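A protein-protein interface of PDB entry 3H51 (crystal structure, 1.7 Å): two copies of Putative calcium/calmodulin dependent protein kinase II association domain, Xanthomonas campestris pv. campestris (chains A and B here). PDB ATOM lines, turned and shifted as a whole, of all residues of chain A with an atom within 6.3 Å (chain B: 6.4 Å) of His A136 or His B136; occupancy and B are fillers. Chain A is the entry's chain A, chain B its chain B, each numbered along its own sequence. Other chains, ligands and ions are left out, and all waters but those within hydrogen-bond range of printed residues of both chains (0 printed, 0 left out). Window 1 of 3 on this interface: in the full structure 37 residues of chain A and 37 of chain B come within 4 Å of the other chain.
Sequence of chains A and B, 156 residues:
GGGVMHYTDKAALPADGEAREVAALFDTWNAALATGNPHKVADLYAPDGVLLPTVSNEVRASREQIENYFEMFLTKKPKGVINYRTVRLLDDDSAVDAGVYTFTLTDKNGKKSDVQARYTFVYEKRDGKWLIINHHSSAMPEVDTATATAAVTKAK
The guanidinium group (NH1) of Arg B118 is in hydrogen-bond range of the backbone carbonyl oxygen (O) of Pro A53 (2.7 Å). The backbone carbonyl oxygen (O) of Pro B53 lies within hydrogen-bond range of the guanidinium group (NH1) of Arg A118 (2.8 Å). NH2 of Arg A118 lies within hydrogen-bond range of O of Ser B137, at 3.0 Å. OG1 of Thr A120 is in hydrogen-bond range of ND2 of Asn B134 (2.8 Å). A ring nitrogen (ND1) of His B136 sits at hydrogen-bond distance from the side-chain hydroxyl of Thr A120, at 3.0 Å. The side-chain amide nitrogen (ND2) of Asn A134 is in hydrogen-bond range of the side-chain hydroxyl (OG1) of Thr B120 (2.8 Å). ND1 of His A136 sits at hydrogen-bond distance from OG1 of Thr B120, at 3.0 Å. OG of Ser B138 sits at hydrogen-bond distance from NE2 of His A136, 2.7 Å away. O of Ser A137 is in hydrogen-bond range of NH2 of Arg B118. The side-chain hydroxyl (OG) of Ser A138 lies within hydrogen-bond range of a ring nitrogen (NE2) of His B136 (2.7 Å).
The backbone NH of Ser A137 is in hydrogen-bond range of the backbone carbonyl oxygen of Leu A52 (2.9 Å). O of Gly A99 lies within hydrogen-bond range of N of Tyr A119 (2.8 Å). The side-chain hydroxyl (OG) of Ser A137 lies within hydrogen-bond range of the side-chain hydroxyl (OH) of Tyr A101. The backbone carbonyl oxygen (O) of Leu B52 is in hydrogen-bond range of the backbone NH (N) of Ser B137, at 2.8 Å. OG1 of Thr B54 lies within hydrogen-bond range of OG of Ser B137, 2.6 Å away. The backbone NH (N) of Arg B118 is in hydrogen-bond range of the backbone carbonyl oxygen (O) of Ser B138 (2.7 Å).
Among the printed residues, pairs that only touch across the chains: Ser A138 with Ser B138 (3.1 Å), Asn A134 with Ala B98 (3.3 Å), Gly A99 with Leu B52 (3.3 Å), His A136 with His B136 (3.3 Å), His A136 with Arg B118 (3.5 Å), Arg A118 with His B136 (3.5 Å), Leu A52 with Gly B99 (3.5 Å), Leu A52 with Arg B118 (3.6 Å), Tyr A119 with Leu B52 (3.6 Å), Arg A118 with Leu B52 (3.6 Å), Leu A52 with Tyr B119 (3.7 Å), Tyr A119 with His B136 (3.7 Å), Arg A118 with Ser B138 (3.7 Å), His A136 with Tyr B119 (3.7 Å), Ser A138 with Arg B118 (3.8 Å), Thr A120 with Leu B52 (3.8 Å) and Leu A52 with Thr B120 (3.8 Å).
Of chain B, only Arg B118, Tyr B119, Thr B120, His B136 and Ser B138 come within 4 Å of His A136. Of chain A, only Arg A118, Tyr A119, Thr A120, His A136 and Ser A138 come within 4 Å of His B136. Printed residues of chain B within 4 Å of Pro A53: Arg B118. Of the printed residues of chain A, Ser B138 touches Arg A118, His A136 and Ser A138. Of the printed residues of chain B, Tyr A119 touches Leu B52 and His B136. The nearest residue of chain A that does not touch His B136 is Ser A137 (4.3 Å). The nearest printed residue of chain B that does not touch Tyr A119 is Asn B134 (5.4 Å).
Of the 16 printed residues of chain A, 10 touch a printed residue of chain B. Printed residues of chain A that touch a printed residue of chain B: Leu A52, Pro A53, Gly A99, Arg A118, Tyr A119, Thr A120, Asn A134, His A136, Ser A137 and Ser A138. Hydrophobic or aromatic side chains of chain A within 4 Å of the printed part of chain B: Leu A52, Pro A53 and His A136. Along chain A the printed residues that touch a printed residue of chain B span positions 52 to 138. Hydrophobic or aromatic side chains of chain B that line the printed part of chain A: Leu B52, Ala B98 and His B136. Among the printed residues, 27 pairs touch across the chains. Among the printed residues, no Asp or Glu carboxylate lies within 4 Å of a Lys or Arg side-chain nitrogen of the other chain.
Leu A52 touches Arg B118, and with the chains exchanged Arg A118 touches Leu B52. Arg A118 touches His B136, and with the chains exchanged His A136 touches Arg B118. Tyr A119 touches His B136, and with the chains exchanged His A136 touches Tyr B119. His A136 touches Ser B138, and with the chains exchanged Ser A138 touches His B136.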
ATOM      1  N   VAL A  50      24.895  -0.268  -8.315  1.00  0.00           N
ATOM      2  CA  VAL A  50      25.921   0.758  -8.586  1.00  0.00           C
ATOM      3  C   VAL A  50      25.315   1.769  -9.581  1.00  0.00           C
ATOM      4  O   VAL A  50      24.852   1.403 -10.640  1.00  0.00           O
ATOM      5  CB  VAL A  50      27.261   0.143  -9.118  1.00  0.00           C
ATOM      6  CG1 VAL A  50      28.335   1.195  -9.378  1.00  0.00           C
ATOM      7  CG2 VAL A  50      27.791  -1.041  -8.195  1.00  0.00           C
ATOM      8  N   LEU A  51      25.316   3.037  -9.186  1.00  0.00           N
ATOM      9  CA  LEU A  51      24.876   4.172  -9.993  1.00  0.00           C
ATOM     10  C   LEU A  51      26.066   5.086 -10.415  1.00  0.00           C
ATOM     11  O   LEU A  51      26.854   5.555  -9.575  1.00  0.00           O
ATOM     12  CB  LEU A  51      23.842   4.972  -9.190  1.00  0.00           C
ATOM     13  CG  LEU A  51      23.357   6.322  -9.718  1.00  0.00           C
ATOM     14  CD1 LEU A  51      22.559   6.143 -11.047  1.00  0.00           C
ATOM     15  CD2 LEU A  51      22.524   7.156  -8.680  1.00  0.00           C
ATOM     16  N   LEU A  52      26.175   5.345 -11.695  1.00  0.00           N
ATOM     17  CA  LEU A  52      27.185   6.186 -12.306  1.00  0.00           C
ATOM     18  C   LEU A  52      26.372   7.288 -12.992  1.00  0.00           C
ATOM     19  O   LEU A  52      25.922   7.127 -14.118  1.00  0.00           O
ATOM     20  CB  LEU A  52      28.044   5.361 -13.275  1.00  0.00           C
ATOM     21  CG  LEU A  52      28.621   4.065 -12.662  1.00  0.00           C
ATOM     22  CD1 LEU A  52      27.808   2.826 -12.956  1.00  0.00           C
ATOM     23  CD2 LEU A  52      30.021   3.879 -13.135  1.00  0.00           C
ATOM     24  N   PRO A  53      26.059   8.338 -12.202  1.00  0.00           N
ATOM     25  CA  PRO A  53      24.989   9.262 -12.524  1.00  0.00           C
ATOM     26  C   PRO A  53      25.339  10.385 -13.485  1.00  0.00           C
ATOM     27  O   PRO A  53      26.530  10.629 -13.777  1.00  0.00           O
ATOM     28  CB  PRO A  53      24.623   9.818 -11.164  1.00  0.00           C
ATOM     29  CG  PRO A  53      25.847   9.862 -10.466  1.00  0.00           C
ATOM     30  CD  PRO A  53      26.626   8.642 -10.876  1.00  0.00           C
ATOM     31  N   THR A  54      24.321  11.037 -14.039  1.00  0.00           N
ATOM     32  CA  THR A  54      24.533  12.065 -15.035  1.00  0.00           C
ATOM     33  C   THR A  54      25.403  13.213 -14.559  1.00  0.00           C
ATOM     34  O   THR A  54      26.305  13.649 -15.299  1.00  0.00           O
ATOM     35  CB  THR A  54      23.178  12.616 -15.574  1.00  0.00           C
ATOM     36  OG1 THR A  54      22.197  11.565 -15.672  1.00  0.00           O
ATOM     37  CG2 THR A  54      23.360  13.163 -16.976  1.00  0.00           C
ATOM     38  N   GLY A  99      19.971   2.773 -23.957  1.00  0.00           N
ATOM     39  CA  GLY A  99      19.668   3.641 -25.089  1.00  0.00           C
ATOM     40  C   GLY A  99      19.865   5.096 -24.764  1.00  0.00           C
ATOM     41  O   GLY A  99      20.847   5.473 -24.102  1.00  0.00           O
ATOM     42  N   TYR A 101      17.650   8.633 -23.502  1.00  0.00           N
ATOM     43  CA  TYR A 101      16.472   9.265 -22.992  1.00  0.00           C
ATOM     44  C   TYR A 101      16.686  10.771 -22.790  1.00  0.00           C
ATOM     45  O   TYR A 101      17.839  11.254 -22.803  1.00  0.00           O
ATOM     46  CB  TYR A 101      16.008   8.549 -21.713  1.00  0.00           C
ATOM     47  CG  TYR A 101      16.945   8.394 -20.485  1.00  0.00           C
ATOM     48  CD1 TYR A 101      18.180   9.070 -20.359  1.00  0.00           C
ATOM     49  CD2 TYR A 101      16.571   7.570 -19.457  1.00  0.00           C
ATOM     50  CE1 TYR A 101      18.997   8.909 -19.245  1.00  0.00           C
ATOM     51  CE2 TYR A 101      17.369   7.408 -18.312  1.00  0.00           C
ATOM     52  CZ  TYR A 101      18.573   8.062 -18.210  1.00  0.00           C
ATOM     53  OH  TYR A 101      19.335   7.845 -17.070  1.00  0.00           O
ATOM     54  N   ARG A 118      22.593   9.299 -22.551  1.00  0.00           N
ATOM     55  CA  ARG A 118      22.615   7.858 -22.772  1.00  0.00           C
ATOM     56  C   ARG A 118      22.354   7.172 -21.420  1.00  0.00           C
ATOM     57  O   ARG A 118      22.712   7.720 -20.322  1.00  0.00           O
ATOM     58  CB  ARG A 118      23.957   7.369 -23.325  1.00  0.00           C
ATOM     59  CG  ARG A 118      24.448   8.005 -24.649  1.00  0.00           C
ATOM     60  CD  ARG A 118      25.225   9.277 -24.454  1.00  0.00           C
ATOM     61  NE  ARG A 118      26.407   9.099 -23.599  1.00  0.00           N
ATOM     62  CZ  ARG A 118      27.557   8.564 -23.982  1.00  0.00           C
ATOM     63  NH1 ARG A 118      27.707   8.059 -25.194  1.00  0.00           N
ATOM     64  NH2 ARG A 118      28.563   8.481 -23.127  1.00  0.00           N
ATOM     65  N   TYR A 119      21.786   5.966 -21.482  1.00  0.00           N
ATOM     66  CA  TYR A 119      21.556   5.150 -20.312  1.00  0.00           C
ATOM     67  C   TYR A 119      21.866   3.674 -20.507  1.00  0.00           C
ATOM     68  O   TYR A 119      21.687   3.119 -21.568  1.00  0.00           O
ATOM     69  CB  TYR A 119      20.112   5.335 -19.776  1.00  0.00           C
ATOM     70  CG  TYR A 119      19.037   4.658 -20.625  1.00  0.00           C
ATOM     71  CD1 TYR A 119      18.639   3.338 -20.369  1.00  0.00           C
ATOM     72  CD2 TYR A 119      18.375   5.327 -21.627  1.00  0.00           C
ATOM     73  CE1 TYR A 119      17.654   2.694 -21.094  1.00  0.00           C
ATOM     74  CE2 TYR A 119      17.390   4.685 -22.390  1.00  0.00           C
ATOM     75  CZ  TYR A 119      17.038   3.354 -22.137  1.00  0.00           C
ATOM     76  OH  TYR A 119      16.035   2.750 -22.885  1.00  0.00           O
ATOM     77  N   THR A 120      22.245   3.059 -19.401  1.00  0.00           N
ATOM     78  CA  THR A 120      22.176   1.631 -19.213  1.00  0.00           C
ATOM     79  C   THR A 120      21.510   1.378 -17.875  1.00  0.00           C
ATOM     80  O   THR A 120      21.990   1.903 -16.868  1.00  0.00           O
ATOM     81  CB  THR A 120      23.571   1.006 -19.175  1.00  0.00           C
ATOM     82  OG1 THR A 120      24.272   1.325 -20.412  1.00  0.00           O
ATOM     83  CG2 THR A 120      23.555  -0.543 -18.891  1.00  0.00           C
ATOM     84  N   PHE A 121      20.444   0.590 -17.895  1.00  0.00           N
ATOM     85  CA  PHE A 121      19.934  -0.121 -16.686  1.00  0.00           C
ATOM     86  C   PHE A 121      20.215  -1.638 -16.805  1.00  0.00           C
ATOM     87  O   PHE A 121      19.840  -2.257 -17.769  1.00  0.00           O
ATOM     88  CB  PHE A 121      18.426   0.050 -16.540  1.00  0.00           C
ATOM     89  CG  PHE A 121      17.985   1.439 -16.202  1.00  0.00           C
ATOM     90  CD1 PHE A 121      17.965   1.865 -14.859  1.00  0.00           C
ATOM     91  CD2 PHE A 121      17.508   2.301 -17.218  1.00  0.00           C
ATOM     92  CE1 PHE A 121      17.510   3.130 -14.547  1.00  0.00           C
ATOM     93  CE2 PHE A 121      17.022   3.561 -16.890  1.00  0.00           C
ATOM     94  CZ  PHE A 121      17.063   3.973 -15.561  1.00  0.00           C
ATOM     95  N   ASN A 134      22.953  -2.067 -11.967  1.00  0.00           N
ATOM     96  CA  ASN A 134      23.786  -1.018 -12.560  1.00  0.00           C
ATOM     97  C   ASN A 134      22.868  -0.010 -13.221  1.00  0.00           C
ATOM     98  O   ASN A 134      21.970  -0.385 -14.021  1.00  0.00           O
ATOM     99  CB  ASN A 134      24.750  -1.561 -13.617  1.00  0.00           C
ATOM    100  CG  ASN A 134      25.884  -0.598 -13.936  1.00  0.00           C
ATOM    101  OD1 ASN A 134      26.879  -0.494 -13.144  1.00  0.00           O
ATOM    102  ND2 ASN A 134      25.736   0.145 -15.001  1.00  0.00           N
ATOM    103  N   HIS A 135      23.121   1.265 -12.950  1.00  0.00           N
ATOM    104  CA  HIS A 135      22.515   2.360 -13.782  1.00  0.00           C
ATOM    105  C   HIS A 135      23.648   3.349 -14.103  1.00  0.00           C
ATOM    106  O   HIS A 135      24.289   3.900 -13.185  1.00  0.00           O
ATOM    107  CB  HIS A 135      21.416   3.041 -12.950  1.00  0.00           C
ATOM    108  CG  HIS A 135      20.743   4.210 -13.612  1.00  0.00           C
ATOM    109  ND1 HIS A 135      19.882   5.042 -12.910  1.00  0.00           N
ATOM    110  CD2 HIS A 135      20.719   4.629 -14.904  1.00  0.00           C
ATOM    111  CE1 HIS A 135      19.401   5.948 -13.743  1.00  0.00           C
ATOM    112  NE2 HIS A 135      19.908   5.735 -14.951  1.00  0.00           N
ATOM    113  N   HIS A 136      23.935   3.519 -15.387  1.00  0.00           N
ATOM    114  CA  HIS A 136      24.926   4.430 -15.866  1.00  0.00           C
ATOM    115  C   HIS A 136      24.134   5.422 -16.724  1.00  0.00           C
ATOM    116  O   HIS A 136      23.356   5.002 -17.598  1.00  0.00           O
ATOM    117  CB  HIS A 136      25.967   3.645 -16.665  1.00  0.00           C
ATOM    118  CG  HIS A 136      27.203   4.410 -17.045  1.00  0.00           C
ATOM    119  ND1 HIS A 136      28.408   3.774 -17.230  1.00  0.00           N
ATOM    120  CD2 HIS A 136      27.411   5.716 -17.363  1.00  0.00           C
ATOM    121  CE1 HIS A 136      29.328   4.673 -17.570  1.00  0.00           C
ATOM    122  NE2 HIS A 136      28.742   5.852 -17.687  1.00  0.00           N
ATOM    123  N   SER A 137      24.284   6.708 -16.436  1.00  0.00           N
ATOM    124  CA  SER A 137      23.525   7.766 -17.157  1.00  0.00           C
ATOM    125  C   SER A 137      24.541   8.861 -17.499  1.00  0.00           C
ATOM    126  O   SER A 137      25.363   9.294 -16.626  1.00  0.00           O
ATOM    127  CB  SER A 137      22.422   8.300 -16.251  1.00  0.00           C
ATOM    128  OG  SER A 137      21.599   9.168 -17.007  1.00  0.00           O
ATOM    129  N   SER A 138      24.586   9.310 -18.765  1.00  0.00           N
ATOM    130  CA  SER A 138      25.638  10.194 -19.174  1.00  0.00           C
ATOM    131  C   SER A 138      25.174  11.193 -20.242  1.00  0.00           C
ATOM    132  O   SER A 138      24.466  10.828 -21.192  1.00  0.00           O
ATOM    133  CB  SER A 138      26.905   9.454 -19.644  1.00  0.00           C
ATOM    134  OG  SER A 138      26.677   8.731 -20.814  1.00  0.00           O
ATOM    135  N   VAL B  50      25.817  -3.668 -27.345  1.00  0.00           N
ATOM    136  CA  VAL B  50      25.471  -2.264 -27.438  1.00  0.00           C
ATOM    137  C   VAL B  50      26.562  -1.436 -26.751  1.00  0.00           C
ATOM    138  O   VAL B  50      26.904  -1.699 -25.606  1.00  0.00           O
ATOM    139  CB  VAL B  50      24.123  -1.967 -26.805  1.00  0.00           C
ATOM    140  CG1 VAL B  50      23.709  -0.480 -26.983  1.00  0.00           C
ATOM    141  CG2 VAL B  50      23.062  -2.891 -27.493  1.00  0.00           C
ATOM    142  N   LEU B  51      27.114  -0.495 -27.508  1.00  0.00           N
ATOM    143  CA  LEU B  51      28.190   0.401 -27.047  1.00  0.00           C
ATOM    144  C   LEU B  51      27.672   1.823 -27.029  1.00  0.00           C
ATOM    145  O   LEU B  51      27.174   2.320 -28.063  1.00  0.00           O
ATOM    146  CB  LEU B  51      29.387   0.267 -27.985  1.00  0.00           C
ATOM    147  CG  LEU B  51      30.508   1.283 -27.843  1.00  0.00           C
ATOM    148  CD1 LEU B  51      31.249   1.163 -26.493  1.00  0.00           C
ATOM    149  CD2 LEU B  51      31.510   1.167 -29.045  1.00  0.00           C
ATOM    150  N   LEU B  52      27.799   2.476 -25.882  1.00  0.00           N
ATOM    151  CA  LEU B  52      27.409   3.870 -25.670  1.00  0.00           C
ATOM    152  C   LEU B  52      28.736   4.572 -25.323  1.00  0.00           C
ATOM    153  O   LEU B  52      29.207   4.523 -24.183  1.00  0.00           O
ATOM    154  CB  LEU B  52      26.304   4.045 -24.632  1.00  0.00           C
ATOM    155  CG  LEU B  52      25.053   3.148 -24.826  1.00  0.00           C
ATOM    156  CD1 LEU B  52      25.150   1.749 -24.062  1.00  0.00           C
ATOM    157  CD2 LEU B  52      23.745   3.840 -24.442  1.00  0.00           C
ATOM    158  N   PRO B  53      29.411   5.087 -26.383  1.00  0.00           N
ATOM    159  CA  PRO B  53      30.843   5.303 -26.189  1.00  0.00           C
ATOM    160  C   PRO B  53      31.252   6.652 -25.633  1.00  0.00           C
ATOM    161  O   PRO B  53      30.462   7.580 -25.571  1.00  0.00           O
ATOM    162  CB  PRO B  53      31.382   5.109 -27.607  1.00  0.00           C
ATOM    163  CG  PRO B  53      30.361   5.617 -28.477  1.00  0.00           C
ATOM    164  CD  PRO B  53      29.028   5.283 -27.797  1.00  0.00           C
ATOM    165  N   THR B  54      32.538   6.755 -25.274  1.00  0.00           N
ATOM    166  CA  THR B  54      33.039   7.956 -24.663  1.00  0.00           C
ATOM    167  C   THR B  54      32.889   9.255 -25.480  1.00  0.00           C
ATOM    168  O   THR B  54      32.499  10.298 -24.931  1.00  0.00           O
ATOM    169  CB  THR B  54      34.566   7.782 -24.294  1.00  0.00           C
ATOM    170  OG1 THR B  54      34.805   6.473 -23.766  1.00  0.00           O
ATOM    171  CG2 THR B  54      34.886   8.822 -23.190  1.00  0.00           C
ATOM    172  N   ALA B  98      31.890  -2.360 -13.357  1.00  0.00           N
ATOM    173  CA  ALA B  98      31.601  -0.925 -13.496  1.00  0.00           C
ATOM    174  C   ALA B  98      32.477  -0.122 -12.528  1.00  0.00           C
ATOM    175  O   ALA B  98      32.823  -0.533 -11.388  1.00  0.00           O
ATOM    176  CB  ALA B  98      30.169  -0.658 -13.178  1.00  0.00           C
ATOM    177  N   GLY B  99      32.815   1.082 -12.982  1.00  0.00           N
ATOM    178  CA  GLY B  99      33.643   1.981 -12.164  1.00  0.00           C
ATOM    179  C   GLY B  99      34.185   3.158 -12.902  1.00  0.00           C
ATOM    180  O   GLY B  99      33.474   3.742 -13.671  1.00  0.00           O
ATOM    181  N   TYR B 101      37.743   4.614 -15.041  1.00  0.00           N
ATOM    182  CA  TYR B 101      39.033   4.323 -15.647  1.00  0.00           C
ATOM    183  C   TYR B 101      39.588   5.544 -16.369  1.00  0.00           C
ATOM    184  O   TYR B 101      38.866   6.515 -16.611  1.00  0.00           O
ATOM    185  CB  TYR B 101      38.999   3.088 -16.598  1.00  0.00           C
ATOM    186  CG  TYR B 101      38.005   3.029 -17.785  1.00  0.00           C
ATOM    187  CD1 TYR B 101      37.272   4.139 -18.244  1.00  0.00           C
ATOM    188  CD2 TYR B 101      37.849   1.802 -18.479  1.00  0.00           C
ATOM    189  CE1 TYR B 101      36.385   4.017 -19.337  1.00  0.00           C
ATOM    190  CE2 TYR B 101      36.984   1.691 -19.583  1.00  0.00           C
ATOM    191  CZ  TYR B 101      36.248   2.810 -20.002  1.00  0.00           C
ATOM    192  OH  TYR B 101      35.368   2.680 -21.119  1.00  0.00           O
ATOM    193  N   ALA B 117      37.041   8.556 -17.151  1.00  0.00           N
ATOM    194  CA  ALA B 117      35.675   8.247 -17.572  1.00  0.00           C
ATOM    195  C   ALA B 117      35.060   7.207 -16.645  1.00  0.00           C
ATOM    196  O   ALA B 117      35.787   6.391 -16.011  1.00  0.00           O
ATOM    197  CB  ALA B 117      35.669   7.761 -19.078  1.00  0.00           C
ATOM    198  N   ARG B 118      33.723   7.206 -16.527  1.00  0.00           N
ATOM    199  CA  ARG B 118      33.075   6.105 -15.833  1.00  0.00           C
ATOM    200  C   ARG B 118      32.849   4.999 -16.896  1.00  0.00           C
ATOM    201  O   ARG B 118      32.687   5.311 -18.079  1.00  0.00           O
ATOM    202  CB  ARG B 118      31.707   6.515 -15.275  1.00  0.00           C
ATOM    203  CG  ARG B 118      31.746   7.645 -14.251  1.00  0.00           C
ATOM    204  CD  ARG B 118      31.676   9.085 -14.834  1.00  0.00           C
ATOM    205  NE  ARG B 118      30.509   9.277 -15.709  1.00  0.00           N
ATOM    206  CZ  ARG B 118      29.257   9.477 -15.274  1.00  0.00           C
ATOM    207  NH1 ARG B 118      28.988   9.535 -13.963  1.00  0.00           N
ATOM    208  NH2 ARG B 118      28.280   9.611 -16.158  1.00  0.00           N
ATOM    209  N   TYR B 119      32.769   3.741 -16.468  1.00  0.00           N
ATOM    210  CA  TYR B 119      32.460   2.650 -17.361  1.00  0.00           C
ATOM    211  C   TYR B 119      31.459   1.646 -16.731  1.00  0.00           C
ATOM    212  O   TYR B 119      31.449   1.457 -15.485  1.00  0.00           O
ATOM    213  CB  TYR B 119      33.765   1.974 -17.813  1.00  0.00           C
ATOM    214  CG  TYR B 119      34.393   1.108 -16.730  1.00  0.00           C
ATOM    215  CD1 TYR B 119      34.082  -0.237 -16.636  1.00  0.00           C
ATOM    216  CD2 TYR B 119      35.337   1.623 -15.851  1.00  0.00           C
ATOM    217  CE1 TYR B 119      34.609  -1.040 -15.653  1.00  0.00           C
ATOM    218  CE2 TYR B 119      35.873   0.834 -14.867  1.00  0.00           C
ATOM    219  CZ  TYR B 119      35.527  -0.490 -14.767  1.00  0.00           C
ATOM    220  OH  TYR B 119      36.087  -1.274 -13.791  1.00  0.00           O
ATOM    221  N   THR B 120      30.635   1.034 -17.606  1.00  0.00           N
ATOM    222  CA  THR B 120      29.939  -0.219 -17.350  1.00  0.00           C
ATOM    223  C   THR B 120      30.251  -1.203 -18.466  1.00  0.00           C
ATOM    224  O   THR B 120      30.054  -0.865 -19.610  1.00  0.00           O
ATOM    225  CB  THR B 120      28.412   0.007 -17.290  1.00  0.00           C
ATOM    226  OG1 THR B 120      28.121   0.940 -16.220  1.00  0.00           O
ATOM    227  CG2 THR B 120      27.666  -1.306 -17.119  1.00  0.00           C
ATOM    228  N   PHE B 121      30.780  -2.362 -18.100  1.00  0.00           N
ATOM    229  CA  PHE B 121      30.806  -3.537 -18.951  1.00  0.00           C
ATOM    230  C   PHE B 121      29.830  -4.578 -18.379  1.00  0.00           C
ATOM    231  O   PHE B 121      29.890  -4.930 -17.183  1.00  0.00           O
ATOM    232  CB  PHE B 121      32.171  -4.199 -19.044  1.00  0.00           C
ATOM    233  CG  PHE B 121      33.237  -3.395 -19.744  1.00  0.00           C
ATOM    234  CD1 PHE B 121      33.353  -3.431 -21.118  1.00  0.00           C
ATOM    235  CD2 PHE B 121      34.204  -2.679 -18.978  1.00  0.00           C
ATOM    236  CE1 PHE B 121      34.398  -2.724 -21.783  1.00  0.00           C
ATOM    237  CE2 PHE B 121      35.224  -1.968 -19.611  1.00  0.00           C
ATOM    238  CZ  PHE B 121      35.326  -2.000 -21.024  1.00  0.00           C
ATOM    239  N   ASN B 134      26.841  -5.006 -23.083  1.00  0.00           N
ATOM    240  CA  ASN B 134      26.692  -3.578 -22.947  1.00  0.00           C
ATOM    241  C   ASN B 134      28.036  -2.993 -22.491  1.00  0.00           C
ATOM    242  O   ASN B 134      28.695  -3.514 -21.576  1.00  0.00           O
ATOM    243  CB  ASN B 134      25.669  -3.221 -21.862  1.00  0.00           C
ATOM    244  CG  ASN B 134      25.247  -1.745 -21.909  1.00  0.00           C
ATOM    245  OD1 ASN B 134      24.388  -1.383 -22.727  1.00  0.00           O
ATOM    246  ND2 ASN B 134      25.884  -0.900 -21.116  1.00  0.00           N
ATOM    247  N   HIS B 135      28.418  -1.903 -23.139  1.00  0.00           N
ATOM    248  CA  HIS B 135      29.552  -1.087 -22.741  1.00  0.00           C
ATOM    249  C   HIS B 135      29.144   0.378 -22.803  1.00  0.00           C
ATOM    250  O   HIS B 135      28.799   0.909 -23.859  1.00  0.00           O
ATOM    251  CB  HIS B 135      30.754  -1.364 -23.655  1.00  0.00           C
ATOM    252  CG  HIS B 135      31.965  -0.593 -23.281  1.00  0.00           C
ATOM    253  ND1 HIS B 135      33.071  -0.533 -24.097  1.00  0.00           N
ATOM    254  CD2 HIS B 135      32.239   0.172 -22.188  1.00  0.00           C
ATOM    255  CE1 HIS B 135      34.007   0.159 -23.466  1.00  0.00           C
ATOM    256  NE2 HIS B 135      33.513   0.649 -22.340  1.00  0.00           N
ATOM    257  N   HIS B 136      29.115   1.011 -21.633  1.00  0.00           N
ATOM    258  CA  HIS B 136      28.748   2.407 -21.543  1.00  0.00           C
ATOM    259  C   HIS B 136      29.954   3.110 -20.955  1.00  0.00           C
ATOM    260  O   HIS B 136      30.503   2.649 -19.961  1.00  0.00           O
ATOM    261  CB  HIS B 136      27.551   2.548 -20.619  1.00  0.00           C
ATOM    262  CG  HIS B 136      26.903   3.902 -20.625  1.00  0.00           C
ATOM    263  ND1 HIS B 136      25.573   4.054 -20.320  1.00  0.00           N
ATOM    264  CD2 HIS B 136      27.400   5.154 -20.810  1.00  0.00           C
ATOM    265  CE1 HIS B 136      25.263   5.354 -20.371  1.00  0.00           C
ATOM    266  NE2 HIS B 136      26.362   6.033 -20.656  1.00  0.00           N
ATOM    267  N   SER B 137      30.428   4.148 -21.653  1.00  0.00           N
ATOM    268  CA  SER B 137      31.671   4.820 -21.258  1.00  0.00           C
ATOM    269  C   SER B 137      31.450   6.322 -21.360  1.00  0.00           C
ATOM    270  O   SER B 137      30.906   6.829 -22.397  1.00  0.00           O
ATOM    271  CB  SER B 137      32.798   4.358 -22.139  1.00  0.00           C
ATOM    272  OG  SER B 137      33.988   4.994 -21.785  1.00  0.00           O
ATOM    273  N   SER B 138      31.762   7.060 -20.305  1.00  0.00           N
ATOM    274  CA  SER B 138      31.383   8.453 -20.249  1.00  0.00           C
ATOM    275  C   SER B 138      32.390   9.303 -19.470  1.00  0.00           C
ATOM    276  O   SER B 138      32.818   8.927 -18.377  1.00  0.00           O
ATOM    277  CB  SER B 138      29.947   8.707 -19.679  1.00  0.00           C
ATOM    278  OG  SER B 138      29.791   8.258 -18.348  1.00  0.00           O
